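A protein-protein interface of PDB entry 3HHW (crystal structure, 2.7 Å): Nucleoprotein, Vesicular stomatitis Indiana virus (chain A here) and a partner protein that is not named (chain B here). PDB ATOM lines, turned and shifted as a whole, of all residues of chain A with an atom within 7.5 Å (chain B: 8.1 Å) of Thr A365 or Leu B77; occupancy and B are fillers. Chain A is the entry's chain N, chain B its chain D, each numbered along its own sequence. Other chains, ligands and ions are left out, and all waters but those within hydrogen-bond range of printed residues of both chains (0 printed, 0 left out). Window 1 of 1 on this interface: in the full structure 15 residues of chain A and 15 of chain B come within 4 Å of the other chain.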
ATOM      1  N   THR A 360      -6.373 -28.574 -10.116  1.00  0.00           N
ATOM      2  CA  THR A 360      -6.952 -28.724  -8.778  1.00  0.00           C
ATOM      3  C   THR A 360      -5.860 -28.682  -7.703  1.00  0.00           C
ATOM      4  O   THR A 360      -4.769 -29.229  -7.893  1.00  0.00           O
ATOM      5  CB  THR A 360      -7.774 -30.034  -8.651  1.00  0.00           C
ATOM      6  OG1 THR A 360      -8.607 -30.195  -9.804  1.00  0.00           O
ATOM      7  CG2 THR A 360      -8.655 -30.016  -7.403  1.00  0.00           C
ATOM      8  N   GLY A 361      -6.164 -28.023  -6.586  1.00  0.00           N
ATOM      9  CA  GLY A 361      -5.236 -27.919  -5.462  1.00  0.00           C
ATOM     10  C   GLY A 361      -5.548 -28.902  -4.349  1.00  0.00           C
ATOM     11  O   GLY A 361      -6.149 -29.955  -4.585  1.00  0.00           O
ATOM     12  N   GLY A 362      -5.135 -28.551  -3.133  1.00  0.00           N
ATOM     13  CA  GLY A 362      -5.341 -29.396  -1.958  1.00  0.00           C
ATOM     14  C   GLY A 362      -4.252 -30.440  -1.805  1.00  0.00           C
ATOM     15  O   GLY A 362      -4.503 -31.636  -1.978  1.00  0.00           O
ATOM     16  N   LEU A 363      -3.043 -29.977  -1.479  1.00  0.00           N
ATOM     17  CA  LEU A 363      -1.829 -30.812  -1.396  1.00  0.00           C
ATOM     18  C   LEU A 363      -1.474 -31.499  -2.728  1.00  0.00           C
ATOM     19  O   LEU A 363      -0.475 -32.222  -2.820  1.00  0.00           O
ATOM     20  CB  LEU A 363      -1.916 -31.831  -0.247  1.00  0.00           C
ATOM     21  CG  LEU A 363      -0.585 -32.242   0.394  1.00  0.00           C
ATOM     22  CD1 LEU A 363      -0.234 -31.327   1.564  1.00  0.00           C
ATOM     23  CD2 LEU A 363      -0.626 -33.691   0.844  1.00  0.00           C
ATOM     24  N   THR A 364      -2.287 -31.251  -3.754  1.00  0.00           N
ATOM     25  CA  THR A 364      -2.028 -31.729  -5.111  1.00  0.00           C
ATOM     26  C   THR A 364      -0.910 -30.884  -5.745  1.00  0.00           C
ATOM     27  O   THR A 364      -0.769 -30.829  -6.973  1.00  0.00           O
ATOM     28  CB  THR A 364      -3.316 -31.669  -5.984  1.00  0.00           C
ATOM     29  OG1 THR A 364      -4.467 -31.967  -5.181  1.00  0.00           O
ATOM     30  CG2 THR A 364      -3.250 -32.659  -7.147  1.00  0.00           C
ATOM     31  N   THR A 365      -0.112 -30.239  -4.894  1.00  0.00           N
ATOM     32  CA  THR A 365       0.907 -29.289  -5.342  1.00  0.00           C
ATOM     33  C   THR A 365       2.175 -29.280  -4.470  1.00  0.00           C
ATOM     34  O   THR A 365       2.349 -28.420  -3.603  1.00  0.00           O
ATOM     35  CB  THR A 365       0.311 -27.850  -5.528  1.00  0.00           C
ATOM     36  OG1 THR A 365       1.370 -26.899  -5.683  1.00  0.00           O
ATOM     37  CG2 THR A 365      -0.576 -27.445  -4.341  1.00  0.00           C
ATOM     38  N   ASN A 366       3.051 -30.254  -4.706  1.00  0.00           N
ATOM     39  CA  ASN A 366       4.390 -30.259  -4.118  1.00  0.00           C
ATOM     40  C   ASN A 366       5.388 -29.617  -5.073  1.00  0.00           C
ATOM     41  O   ASN A 366       6.237 -28.821  -4.662  1.00  0.00           O
ATOM     42  CB  ASN A 366       4.839 -31.686  -3.797  1.00  0.00           C
ATOM     43  CG  ASN A 366       6.299 -31.759  -3.368  1.00  0.00           C
ATOM     44  OD1 ASN A 366       6.664 -31.316  -2.277  1.00  0.00           O
ATOM     45  ND2 ASN A 366       7.140 -32.322  -4.228  1.00  0.00           N
ATOM     46  N   ALA A 367       5.265 -29.978  -6.349  1.00  0.00           N
ATOM     47  CA  ALA A 367       6.148 -29.526  -7.418  1.00  0.00           C
ATOM     48  C   ALA A 367       6.259 -27.998  -7.521  1.00  0.00           C
ATOM     49  O   ALA A 367       5.336 -27.281  -7.124  1.00  0.00           O
ATOM     50  CB  ALA A 367       5.685 -30.118  -8.751  1.00  0.00           C
ATOM     51  N   PRO A 368       7.403 -27.499  -8.036  1.00  0.00           N
ATOM     52  CA  PRO A 368       7.600 -26.090  -8.395  1.00  0.00           C
ATOM     53  C   PRO A 368       6.485 -25.523  -9.290  1.00  0.00           C
ATOM     54  O   PRO A 368       5.764 -26.293  -9.934  1.00  0.00           O
ATOM     55  CB  PRO A 368       8.941 -26.102  -9.149  1.00  0.00           C
ATOM     56  CG  PRO A 368       9.274 -27.544  -9.382  1.00  0.00           C
ATOM     57  CD  PRO A 368       8.629 -28.282  -8.270  1.00  0.00           C
ATOM     58  N   PRO A 369       6.345 -24.181  -9.337  1.00  0.00           N
ATOM     59  CA  PRO A 369       5.237 -23.567 -10.069  1.00  0.00           C
ATOM     60  C   PRO A 369       5.332 -23.800 -11.570  1.00  0.00           C
ATOM     61  O   PRO A 369       6.425 -23.967 -12.105  1.00  0.00           O
ATOM     62  CB  PRO A 369       5.399 -22.070  -9.773  1.00  0.00           C
ATOM     63  CG  PRO A 369       6.318 -21.985  -8.613  1.00  0.00           C
ATOM     64  CD  PRO A 369       7.215 -23.163  -8.720  1.00  0.00           C
ATOM     65  N   GLY A 379       7.739 -16.915  -4.253  1.00  0.00           N
ATOM     66  CA  GLY A 379       6.915 -17.583  -3.257  1.00  0.00           C
ATOM     67  C   GLY A 379       7.429 -18.978  -2.979  1.00  0.00           C
ATOM     68  O   GLY A 379       7.596 -19.367  -1.825  1.00  0.00           O
ATOM     69  N   TRP A 380       7.689 -19.721  -4.051  1.00  0.00           N
ATOM     70  CA  TRP A 380       8.188 -21.090  -3.963  1.00  0.00           C
ATOM     71  C   TRP A 380       9.551 -21.162  -3.276  1.00  0.00           C
ATOM     72  O   TRP A 380       9.767 -22.024  -2.423  1.00  0.00           O
ATOM     73  CB  TRP A 380       8.256 -21.710  -5.358  1.00  0.00           C
ATOM     74  CG  TRP A 380       8.799 -23.108  -5.398  1.00  0.00           C
ATOM     75  CD1 TRP A 380       8.108 -24.263  -5.176  1.00  0.00           C
ATOM     76  CD2 TRP A 380      10.146 -23.496  -5.696  1.00  0.00           C
ATOM     77  NE1 TRP A 380       8.940 -25.346  -5.308  1.00  0.00           N
ATOM     78  CE2 TRP A 380      10.197 -24.905  -5.630  1.00  0.00           C
ATOM     79  CE3 TRP A 380      11.314 -22.789  -6.010  1.00  0.00           C
ATOM     80  CZ2 TRP A 380      11.374 -25.625  -5.865  1.00  0.00           C
ATOM     81  CZ3 TRP A 380      12.483 -23.503  -6.245  1.00  0.00           C
ATOM     82  CH2 TRP A 380      12.503 -24.907  -6.171  1.00  0.00           C
ATOM     83  N   ASP A 383       9.448 -20.754   0.379  1.00  0.00           N
ATOM     84  CA  ASP A 383       9.043 -22.020   0.992  1.00  0.00           C
ATOM     85  C   ASP A 383      10.186 -23.037   1.016  1.00  0.00           C
ATOM     86  O   ASP A 383      10.165 -23.988   1.796  1.00  0.00           O
ATOM     87  CB  ASP A 383       7.827 -22.607   0.266  1.00  0.00           C
ATOM     88  CG  ASP A 383       6.571 -21.766   0.438  1.00  0.00           C
ATOM     89  OD1 ASP A 383       6.380 -21.166   1.521  1.00  0.00           O
ATOM     90  OD2 ASP A 383       5.762 -21.712  -0.513  1.00  0.00           O
ATOM     91  N   GLN A 384      11.178 -22.824   0.158  1.00  0.00           N
ATOM     92  CA  GLN A 384      12.370 -23.667   0.107  1.00  0.00           C
ATOM     93  C   GLN A 384      13.474 -23.157   1.045  1.00  0.00           C
ATOM     94  O   GLN A 384      14.647 -23.512   0.885  1.00  0.00           O
ATOM     95  CB  GLN A 384      12.879 -23.756  -1.338  1.00  0.00           C
ATOM     96  CG  GLN A 384      12.526 -25.046  -2.075  1.00  0.00           C
ATOM     97  CD  GLN A 384      11.068 -25.459  -1.939  1.00  0.00           C
ATOM     98  OE1 GLN A 384      10.156 -24.681  -2.211  1.00  0.00           O
ATOM     99  NE2 GLN A 384      10.849 -26.702  -1.528  1.00  0.00           N
ATOM    100  N   LEU B  39      -8.558 -23.366  -3.694  1.00  0.00           N
ATOM    101  CA  LEU B  39      -7.787 -24.361  -2.951  1.00  0.00           C
ATOM    102  C   LEU B  39      -8.576 -24.863  -1.742  1.00  0.00           C
ATOM    103  O   LEU B  39      -8.900 -24.092  -0.836  1.00  0.00           O
ATOM    104  CB  LEU B  39      -6.427 -23.780  -2.531  1.00  0.00           C
ATOM    105  CG  LEU B  39      -5.437 -24.611  -1.705  1.00  0.00           C
ATOM    106  CD1 LEU B  39      -4.018 -24.461  -2.234  1.00  0.00           C
ATOM    107  CD2 LEU B  39      -5.502 -24.231  -0.230  1.00  0.00           C
ATOM    108  N   ILE B  41      -8.267 -27.249   1.352  1.00  0.00           N
ATOM    109  CA  ILE B  41      -7.271 -27.936   2.171  1.00  0.00           C
ATOM    110  C   ILE B  41      -7.810 -28.308   3.561  1.00  0.00           C
ATOM    111  O   ILE B  41      -8.600 -27.567   4.152  1.00  0.00           O
ATOM    112  CB  ILE B  41      -5.945 -27.106   2.266  1.00  0.00           C
ATOM    113  CG1 ILE B  41      -4.762 -27.976   2.713  1.00  0.00           C
ATOM    114  CG2 ILE B  41      -6.112 -25.868   3.153  1.00  0.00           C
ATOM    115  CD1 ILE B  41      -4.153 -28.825   1.609  1.00  0.00           C
ATOM    116  N   LEU B  46      -2.305 -32.178   5.450  1.00  0.00           N
ATOM    117  CA  LEU B  46      -1.084 -31.445   5.785  1.00  0.00           C
ATOM    118  C   LEU B  46      -0.227 -32.121   6.860  1.00  0.00           C
ATOM    119  O   LEU B  46       0.933 -31.750   7.050  1.00  0.00           O
ATOM    120  CB  LEU B  46      -1.428 -30.010   6.210  1.00  0.00           C
ATOM    121  CG  LEU B  46      -2.172 -29.100   5.222  1.00  0.00           C
ATOM    122  CD1 LEU B  46      -2.819 -27.932   5.951  1.00  0.00           C
ATOM    123  CD2 LEU B  46      -1.261 -28.600   4.105  1.00  0.00           C
ATOM    124  N   ILE B  68      -4.145 -24.367  10.135  1.00  0.00           N
ATOM    125  CA  ILE B  68      -4.062 -24.484   8.676  1.00  0.00           C
ATOM    126  C   ILE B  68      -2.901 -23.647   8.129  1.00  0.00           C
ATOM    127  O   ILE B  68      -2.144 -24.114   7.276  1.00  0.00           O
ATOM    128  CB  ILE B  68      -5.409 -24.104   7.977  1.00  0.00           C
ATOM    129  CG1 ILE B  68      -6.504 -25.148   8.265  1.00  0.00           C
ATOM    130  CG2 ILE B  68      -5.225 -23.896   6.462  1.00  0.00           C
ATOM    131  CD1 ILE B  68      -6.254 -26.549   7.703  1.00  0.00           C
ATOM    132  N   LEU B  69      -2.767 -22.419   8.632  1.00  0.00           N
ATOM    133  CA  LEU B  69      -1.667 -21.527   8.250  1.00  0.00           C
ATOM    134  C   LEU B  69      -0.305 -22.052   8.702  1.00  0.00           C
ATOM    135  O   LEU B  69       0.710 -21.792   8.052  1.00  0.00           O
ATOM    136  CB  LEU B  69      -1.902 -20.102   8.770  1.00  0.00           C
ATOM    137  CG  LEU B  69      -2.557 -19.081   7.827  1.00  0.00           C
ATOM    138  CD1 LEU B  69      -4.024 -19.395   7.539  1.00  0.00           C
ATOM    139  CD2 LEU B  69      -2.421 -17.672   8.392  1.00  0.00           C
ATOM    140  N   LEU B  70      -0.289 -22.782   9.816  1.00  0.00           N
ATOM    141  CA  LEU B  70       0.908 -23.493  10.265  1.00  0.00           C
ATOM    142  C   LEU B  70       1.048 -24.813   9.504  1.00  0.00           C
ATOM    143  O   LEU B  70       2.153 -25.343   9.361  1.00  0.00           O
ATOM    144  CB  LEU B  70       0.853 -23.752  11.775  1.00  0.00           C
ATOM    145  CG  LEU B  70       2.093 -24.331  12.471  1.00  0.00           C
ATOM    146  CD1 LEU B  70       3.110 -23.242  12.802  1.00  0.00           C
ATOM    147  CD2 LEU B  70       1.694 -25.088  13.728  1.00  0.00           C
ATOM    148  N   GLY B  71      -0.080 -25.325   9.013  1.00  0.00           N
ATOM    149  CA  GLY B  71      -0.130 -26.589   8.275  1.00  0.00           C
ATOM    150  C   GLY B  71       0.628 -26.600   6.960  1.00  0.00           C
ATOM    151  O   GLY B  71       0.978 -27.668   6.452  1.00  0.00           O
ATOM    152  N   LEU B  72       0.878 -25.417   6.402  1.00  0.00           N
ATOM    153  CA  LEU B  72       1.692 -25.300   5.197  1.00  0.00           C
ATOM    154  C   LEU B  72       3.171 -25.508   5.537  1.00  0.00           C
ATOM    155  O   LEU B  72       3.912 -24.552   5.787  1.00  0.00           O
ATOM    156  CB  LEU B  72       1.464 -23.953   4.492  1.00  0.00           C
ATOM    157  CG  LEU B  72       0.123 -23.561   3.840  1.00  0.00           C
ATOM    158  CD1 LEU B  72      -0.679 -24.755   3.321  1.00  0.00           C
ATOM    159  CD2 LEU B  72      -0.729 -22.727   4.777  1.00  0.00           C
ATOM    160  N   ARG B  73       3.577 -26.777   5.559  1.00  0.00           N
ATOM    161  CA  ARG B  73       4.951 -27.172   5.866  1.00  0.00           C
ATOM    162  C   ARG B  73       5.287 -28.536   5.258  1.00  0.00           C
ATOM    163  O   ARG B  73       6.438 -28.791   4.902  1.00  0.00           O
ATOM    164  CB  ARG B  73       5.175 -27.225   7.380  1.00  0.00           C
ATOM    165  CG  ARG B  73       6.642 -27.236   7.785  1.00  0.00           C
ATOM    166  CD  ARG B  73       6.937 -28.352   8.772  1.00  0.00           C
ATOM    167  NE  ARG B  73       8.358 -28.423   9.107  1.00  0.00           N
ATOM    168  CZ  ARG B  73       8.946 -29.455   9.707  1.00  0.00           C
ATOM    169  NH1 ARG B  73      10.245 -29.416   9.967  1.00  0.00           N
ATOM    170  NH2 ARG B  73       8.245 -30.532  10.043  1.00  0.00           N
ATOM    171  N   TYR B  74       4.278 -29.402   5.152  1.00  0.00           N
ATOM    172  CA  TYR B  74       4.449 -30.777   4.668  1.00  0.00           C
ATOM    173  C   TYR B  74       5.043 -30.848   3.259  1.00  0.00           C
ATOM    174  O   TYR B  74       5.948 -31.647   3.000  1.00  0.00           O
ATOM    175  CB  TYR B  74       3.116 -31.536   4.731  1.00  0.00           C
ATOM    176  CG  TYR B  74       3.175 -32.969   4.232  1.00  0.00           C
ATOM    177  CD1 TYR B  74       2.593 -33.326   3.015  1.00  0.00           C
ATOM    178  CD2 TYR B  74       3.809 -33.965   4.976  1.00  0.00           C
ATOM    179  CE1 TYR B  74       2.641 -34.638   2.550  1.00  0.00           C
ATOM    180  CE2 TYR B  74       3.863 -35.280   4.520  1.00  0.00           C
ATOM    181  CZ  TYR B  74       3.277 -35.608   3.306  1.00  0.00           C
ATOM    182  OH  TYR B  74       3.328 -36.905   2.848  1.00  0.00           O
ATOM    183  N   LYS B  75       4.525 -30.018   2.358  1.00  0.00           N
ATOM    184  CA  LYS B  75       5.057 -29.916   1.000  1.00  0.00           C
ATOM    185  C   LYS B  75       5.823 -28.604   0.811  1.00  0.00           C
ATOM    186  O   LYS B  75       6.340 -28.330  -0.277  1.00  0.00           O
ATOM    187  CB  LYS B  75       3.932 -30.034  -0.040  1.00  0.00           C
ATOM    188  CG  LYS B  75       3.180 -31.369  -0.048  1.00  0.00           C
ATOM    189  CD  LYS B  75       4.062 -32.532  -0.485  1.00  0.00           C
ATOM    190  CE  LYS B  75       3.231 -33.709  -0.963  1.00  0.00           C
ATOM    191  NZ  LYS B  75       4.088 -34.811  -1.480  1.00  0.00           N
ATOM    192  N   LYS B  76       5.904 -27.818   1.890  1.00  0.00           N
ATOM    193  CA  LYS B  76       6.524 -26.483   1.897  1.00  0.00           C
ATOM    194  C   LYS B  76       5.832 -25.560   0.887  1.00  0.00           C
ATOM    195  O   LYS B  76       6.333 -25.339  -0.220  1.00  0.00           O
ATOM    196  CB  LYS B  76       8.045 -26.551   1.648  1.00  0.00           C
ATOM    197  CG  LYS B  76       8.808 -27.572   2.506  1.00  0.00           C
ATOM    198  CD  LYS B  76       9.076 -27.077   3.926  1.00  0.00           C
ATOM    199  CE  LYS B  76      10.426 -26.390   4.044  1.00  0.00           C
ATOM    200  NZ  LYS B  76      10.713 -25.991   5.449  1.00  0.00           N
ATOM    201  N   LEU B  77       4.672 -25.036   1.278  1.00  0.00           N
ATOM    202  CA  LEU B  77       3.831 -24.249   0.374  1.00  0.00           C
ATOM    203  C   LEU B  77       2.996 -23.162   1.061  1.00  0.00           C
ATOM    204  O   LEU B  77       1.779 -23.092   0.872  1.00  0.00           O
ATOM    205  CB  LEU B  77       2.931 -25.161  -0.487  1.00  0.00           C
ATOM    206  CG  LEU B  77       2.362 -26.512  -0.020  1.00  0.00           C
ATOM    207  CD1 LEU B  77       1.878 -26.524   1.428  1.00  0.00           C
ATOM    208  CD2 LEU B  77       1.237 -26.938  -0.951  1.00  0.00           C
ATOM    209  N   TYR B  78       3.652 -22.308   1.845  1.00  0.00           N
ATOM    210  CA  TYR B  78       2.967 -21.183   2.479  1.00  0.00           C
ATOM    211  C   TYR B  78       2.942 -19.949   1.577  1.00  0.00           C
ATOM    212  O   TYR B  78       1.869 -19.488   1.184  1.00  0.00           O
ATOM    213  CB  TYR B  78       3.587 -20.844   3.842  1.00  0.00           C
ATOM    214  CG  TYR B  78       2.958 -19.638   4.519  1.00  0.00           C
ATOM    215  CD1 TYR B  78       1.771 -19.758   5.244  1.00  0.00           C
ATOM    216  CD2 TYR B  78       3.549 -18.377   4.430  1.00  0.00           C
ATOM    217  CE1 TYR B  78       1.191 -18.652   5.862  1.00  0.00           C
ATOM    218  CE2 TYR B  78       2.975 -17.267   5.042  1.00  0.00           C
ATOM    219  CZ  TYR B  78       1.800 -17.412   5.757  1.00  0.00           C
ATOM    220  OH  TYR B  78       1.238 -16.315   6.365  1.00  0.00           O
ATOM    221  N   ASN B  79       4.126 -19.427   1.255  1.00  0.00           N
ATOM    222  CA  ASN B  79       4.255 -18.192   0.480  1.00  0.00           C
ATOM    223  C   ASN B  79       3.768 -18.320  -0.960  1.00  0.00           C
ATOM    224  O   ASN B  79       3.347 -17.333  -1.567  1.00  0.00           O
ATOM    225  CB  ASN B  79       5.699 -17.685   0.503  1.00  0.00           C
ATOM    226  CG  ASN B  79       6.181 -17.363   1.903  1.00  0.00           C
ATOM    227  OD1 ASN B  79       6.436 -18.261   2.704  1.00  0.00           O
ATOM    228  ND2 ASN B  79       6.318 -16.077   2.201  1.00  0.00           N
ATOM    229  N   GLN B  80       3.829 -19.536  -1.498  1.00  0.00           N
ATOM    230  CA  GLN B  80       3.332 -19.812  -2.844  1.00  0.00           C
ATOM    231  C   GLN B  80       1.800 -19.729  -2.896  1.00  0.00           C
ATOM    232  O   GLN B  80       1.232 -19.251  -3.881  1.00  0.00           O
ATOM    233  CB  GLN B  80       3.824 -21.180  -3.331  1.00  0.00           C
ATOM    234  CG  GLN B  80       3.820 -21.342  -4.851  1.00  0.00           C
ATOM    235  CD  GLN B  80       4.163 -22.753  -5.302  1.00  0.00           C
ATOM    236  OE1 GLN B  80       4.985 -23.436  -4.689  1.00  0.00           O
ATOM    237  NE2 GLN B  80       3.532 -23.195  -6.386  1.00  0.00           N
ATOM    238  N   ALA B  81       1.145 -20.186  -1.829  1.00  0.00           N
ATOM    239  CA  ALA B  81      -0.313 -20.126  -1.716  1.00  0.00           C
ATOM    240  C   ALA B  81      -0.800 -18.789  -1.145  1.00  0.00           C
ATOM    241  O   ALA B  81      -1.994 -18.487  -1.191  1.00  0.00           O
ATOM    242  CB  ALA B  81      -0.828 -21.288  -0.874  1.00  0.00           C
ATOM    243  N   ARG B  82       0.134 -17.999  -0.615  1.00  0.00           N
ATOM    244  CA  ARG B  82      -0.167 -16.698  -0.014  1.00  0.00           C
ATOM    245  C   ARG B  82      -0.518 -15.646  -1.069  1.00  0.00           C
ATOM    246  O   ARG B  82      -1.442 -14.852  -0.878  1.00  0.00           O
ATOM    247  CB  ARG B  82       1.015 -16.223   0.847  1.00  0.00           C
ATOM    248  CG  ARG B  82       0.793 -14.929   1.638  1.00  0.00           C
ATOM    249  CD  ARG B  82       0.053 -15.171   2.948  1.00  0.00           C
ATOM    250  NE  ARG B  82       0.151 -14.024   3.850  1.00  0.00           N
ATOM    251  CZ  ARG B  82      -0.387 -13.963   5.067  1.00  0.00           C
ATOM    252  NH1 ARG B  82      -0.233 -12.872   5.805  1.00  0.00           N
ATOM    253  NH2 ARG B  82      -1.080 -14.987   5.553  1.00  0.00           N
ATOM    254  N   LYS B  84      -1.106 -16.470  -4.416  1.00  0.00           N
ATOM    255  CA  LYS B  84      -2.004 -17.073  -5.403  1.00  0.00           C
ATOM    256  C   LYS B  84      -3.460 -17.106  -4.931  1.00  0.00           C
ATOM    257  O   LYS B  84      -4.381 -17.123  -5.751  1.00  0.00           O
ATOM    258  CB  LYS B  84      -1.538 -18.485  -5.771  1.00  0.00           C
ATOM    259  CG  LYS B  84      -0.402 -18.524  -6.788  1.00  0.00           C
ATOM    260  CD  LYS B  84      -0.066 -19.950  -7.224  1.00  0.00           C
ATOM    261  CE  LYS B  84      -1.100 -20.523  -8.194  1.00  0.00           C
ATOM    262  NZ  LYS B  84      -1.106 -19.824  -9.510  1.00  0.00           N
ATOM    263  N   TYR B  85      -3.657 -17.115  -3.614  1.00  0.00           N
ATOM    264  CA  TYR B  85      -4.994 -17.197  -3.022  1.00  0.00           C
ATOM    265  C   TYR B  85      -5.259 -16.062  -2.029  1.00  0.00           C
ATOM    266  O   TYR B  85      -4.328 -15.387  -1.581  1.00  0.00           O
ATOM    267  CB  TYR B  85      -5.203 -18.566  -2.357  1.00  0.00           C
ATOM    268  CG  TYR B  85      -5.091 -19.734  -3.318  1.00  0.00           C
ATOM    269  CD1 TYR B  85      -6.179 -20.132  -4.094  1.00  0.00           C
ATOM    270  CD2 TYR B  85      -3.894 -20.437  -3.453  1.00  0.00           C
ATOM    271  CE1 TYR B  85      -6.078 -21.197  -4.984  1.00  0.00           C
ATOM    272  CE2 TYR B  85      -3.782 -21.505  -4.339  1.00  0.00           C
ATOM    273  CZ  TYR B  85      -4.877 -21.880  -5.100  1.00  0.00           C
ATOM    274  OH  TYR B  85      -4.771 -22.939  -5.975  1.00  0.00           O
ATOM    275  N   LEU B  87      -5.572 -15.936   0.853  1.00  0.00           N
ATOM    276  CA  LEU B  87      -5.016 -16.249   2.164  1.00  0.00           C
ATOM    277  C   LEU B  87      -4.325 -15.019   2.756  1.00  0.00           C
ATOM    278  O   LEU B  87      -4.403 -14.762   3.958  1.00  0.00           O
ATOM    279  CB  LEU B  87      -4.023 -17.411   2.041  1.00  0.00           C
ATOM    280  CG  LEU B  87      -3.783 -18.353   3.226  1.00  0.00           C
ATOM    281  CD1 LEU B  87      -3.294 -19.706   2.722  1.00  0.00           C
ATOM    282  CD2 LEU B  87      -2.801 -17.772   4.241  1.00  0.00           C
ATOM    283  OXT LEU B  87      -3.680 -14.247   2.045  1.00  0.00           O
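The backbone NH (N) of Tyr B78 is in hydrogen-bond range of the side-chain carboxylate (OD1) of Asp A383. The backbone NH (N) of Asn B79 lies within hydrogen-bond range of the side-chain carboxylate (OD1) of Asp A383 (2.9 Å). OD2 of Asp A383 lies within hydrogen-bond range of N of Gln B80 (3.1 Å).
The side-chain hydroxyl of Tyr B78 lies within hydrogen-bond range of the guanidinium group of Arg B82 (2.8 Å). The side-chain hydroxyl (OG1) of Thr A364 is in hydrogen-bond range of the backbone carbonyl oxygen (O) of Gly A362, at 3.2 Å. The backbone carbonyl oxygen of Trp A380 lies close to the side-chain amide oxygen of Gln A384.
Among the printed residues, pairs that only touch across the chains: Gly A362 with Ile B41 (3.8 Å), Leu A363 with Ile B41 (3.5 Å), Leu A363 with Leu B46 (3.9 Å), Leu A363 with Tyr B74 (3.8 Å), Leu A363 with Lys B75 (3.8 Å), Thr A365 with Leu B77 (3.2 Å), Asn A366 with Lys B75 (3.4 Å), Pro A369 with Gln B80 (3.8 Å), Gly A379 with Asn B79 (3.4 Å), Gly A379 with Gln B80 (3.8 Å), Trp A380 with Gln B80 (3.3 Å), Asp A383 with Lys B76 (3.2 Å) and Asp A383 with Leu B77 (3.3 Å).
Thr A365 touches just one residue of chain B: Leu B77 (3.2 Å). Leu B77 touches just these residues of chain A: Thr A365 and Asp A383. Of the printed residues of chain B, Pro A369 touches Gln B80 (3.8 Å). Of the printed residues of chain B, Gly A379 touches Asn B79 (3.4 Å) and Gln B80 (3.8 Å). Leu B69 touches none of the printed residues of chain A. The nearest residue of chain B that does not touch Thr A365 is Lys B75 (4.2 Å).
Of the 21 printed residues of chain B, 9 touch a printed residue of chain A. Hydrophobic or aromatic side chains of chain B that line the printed part of chain A: Ile B41, Leu B46, Tyr B74, Leu B77 and Tyr B78. Along chain B the printed residues that touch a printed residue of chain A span positions 41 to 80. Among the printed residues, no Asp or Glu carboxylate lies within 4 Å of a Lys or Arg side-chain nitrogen of the other chain.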
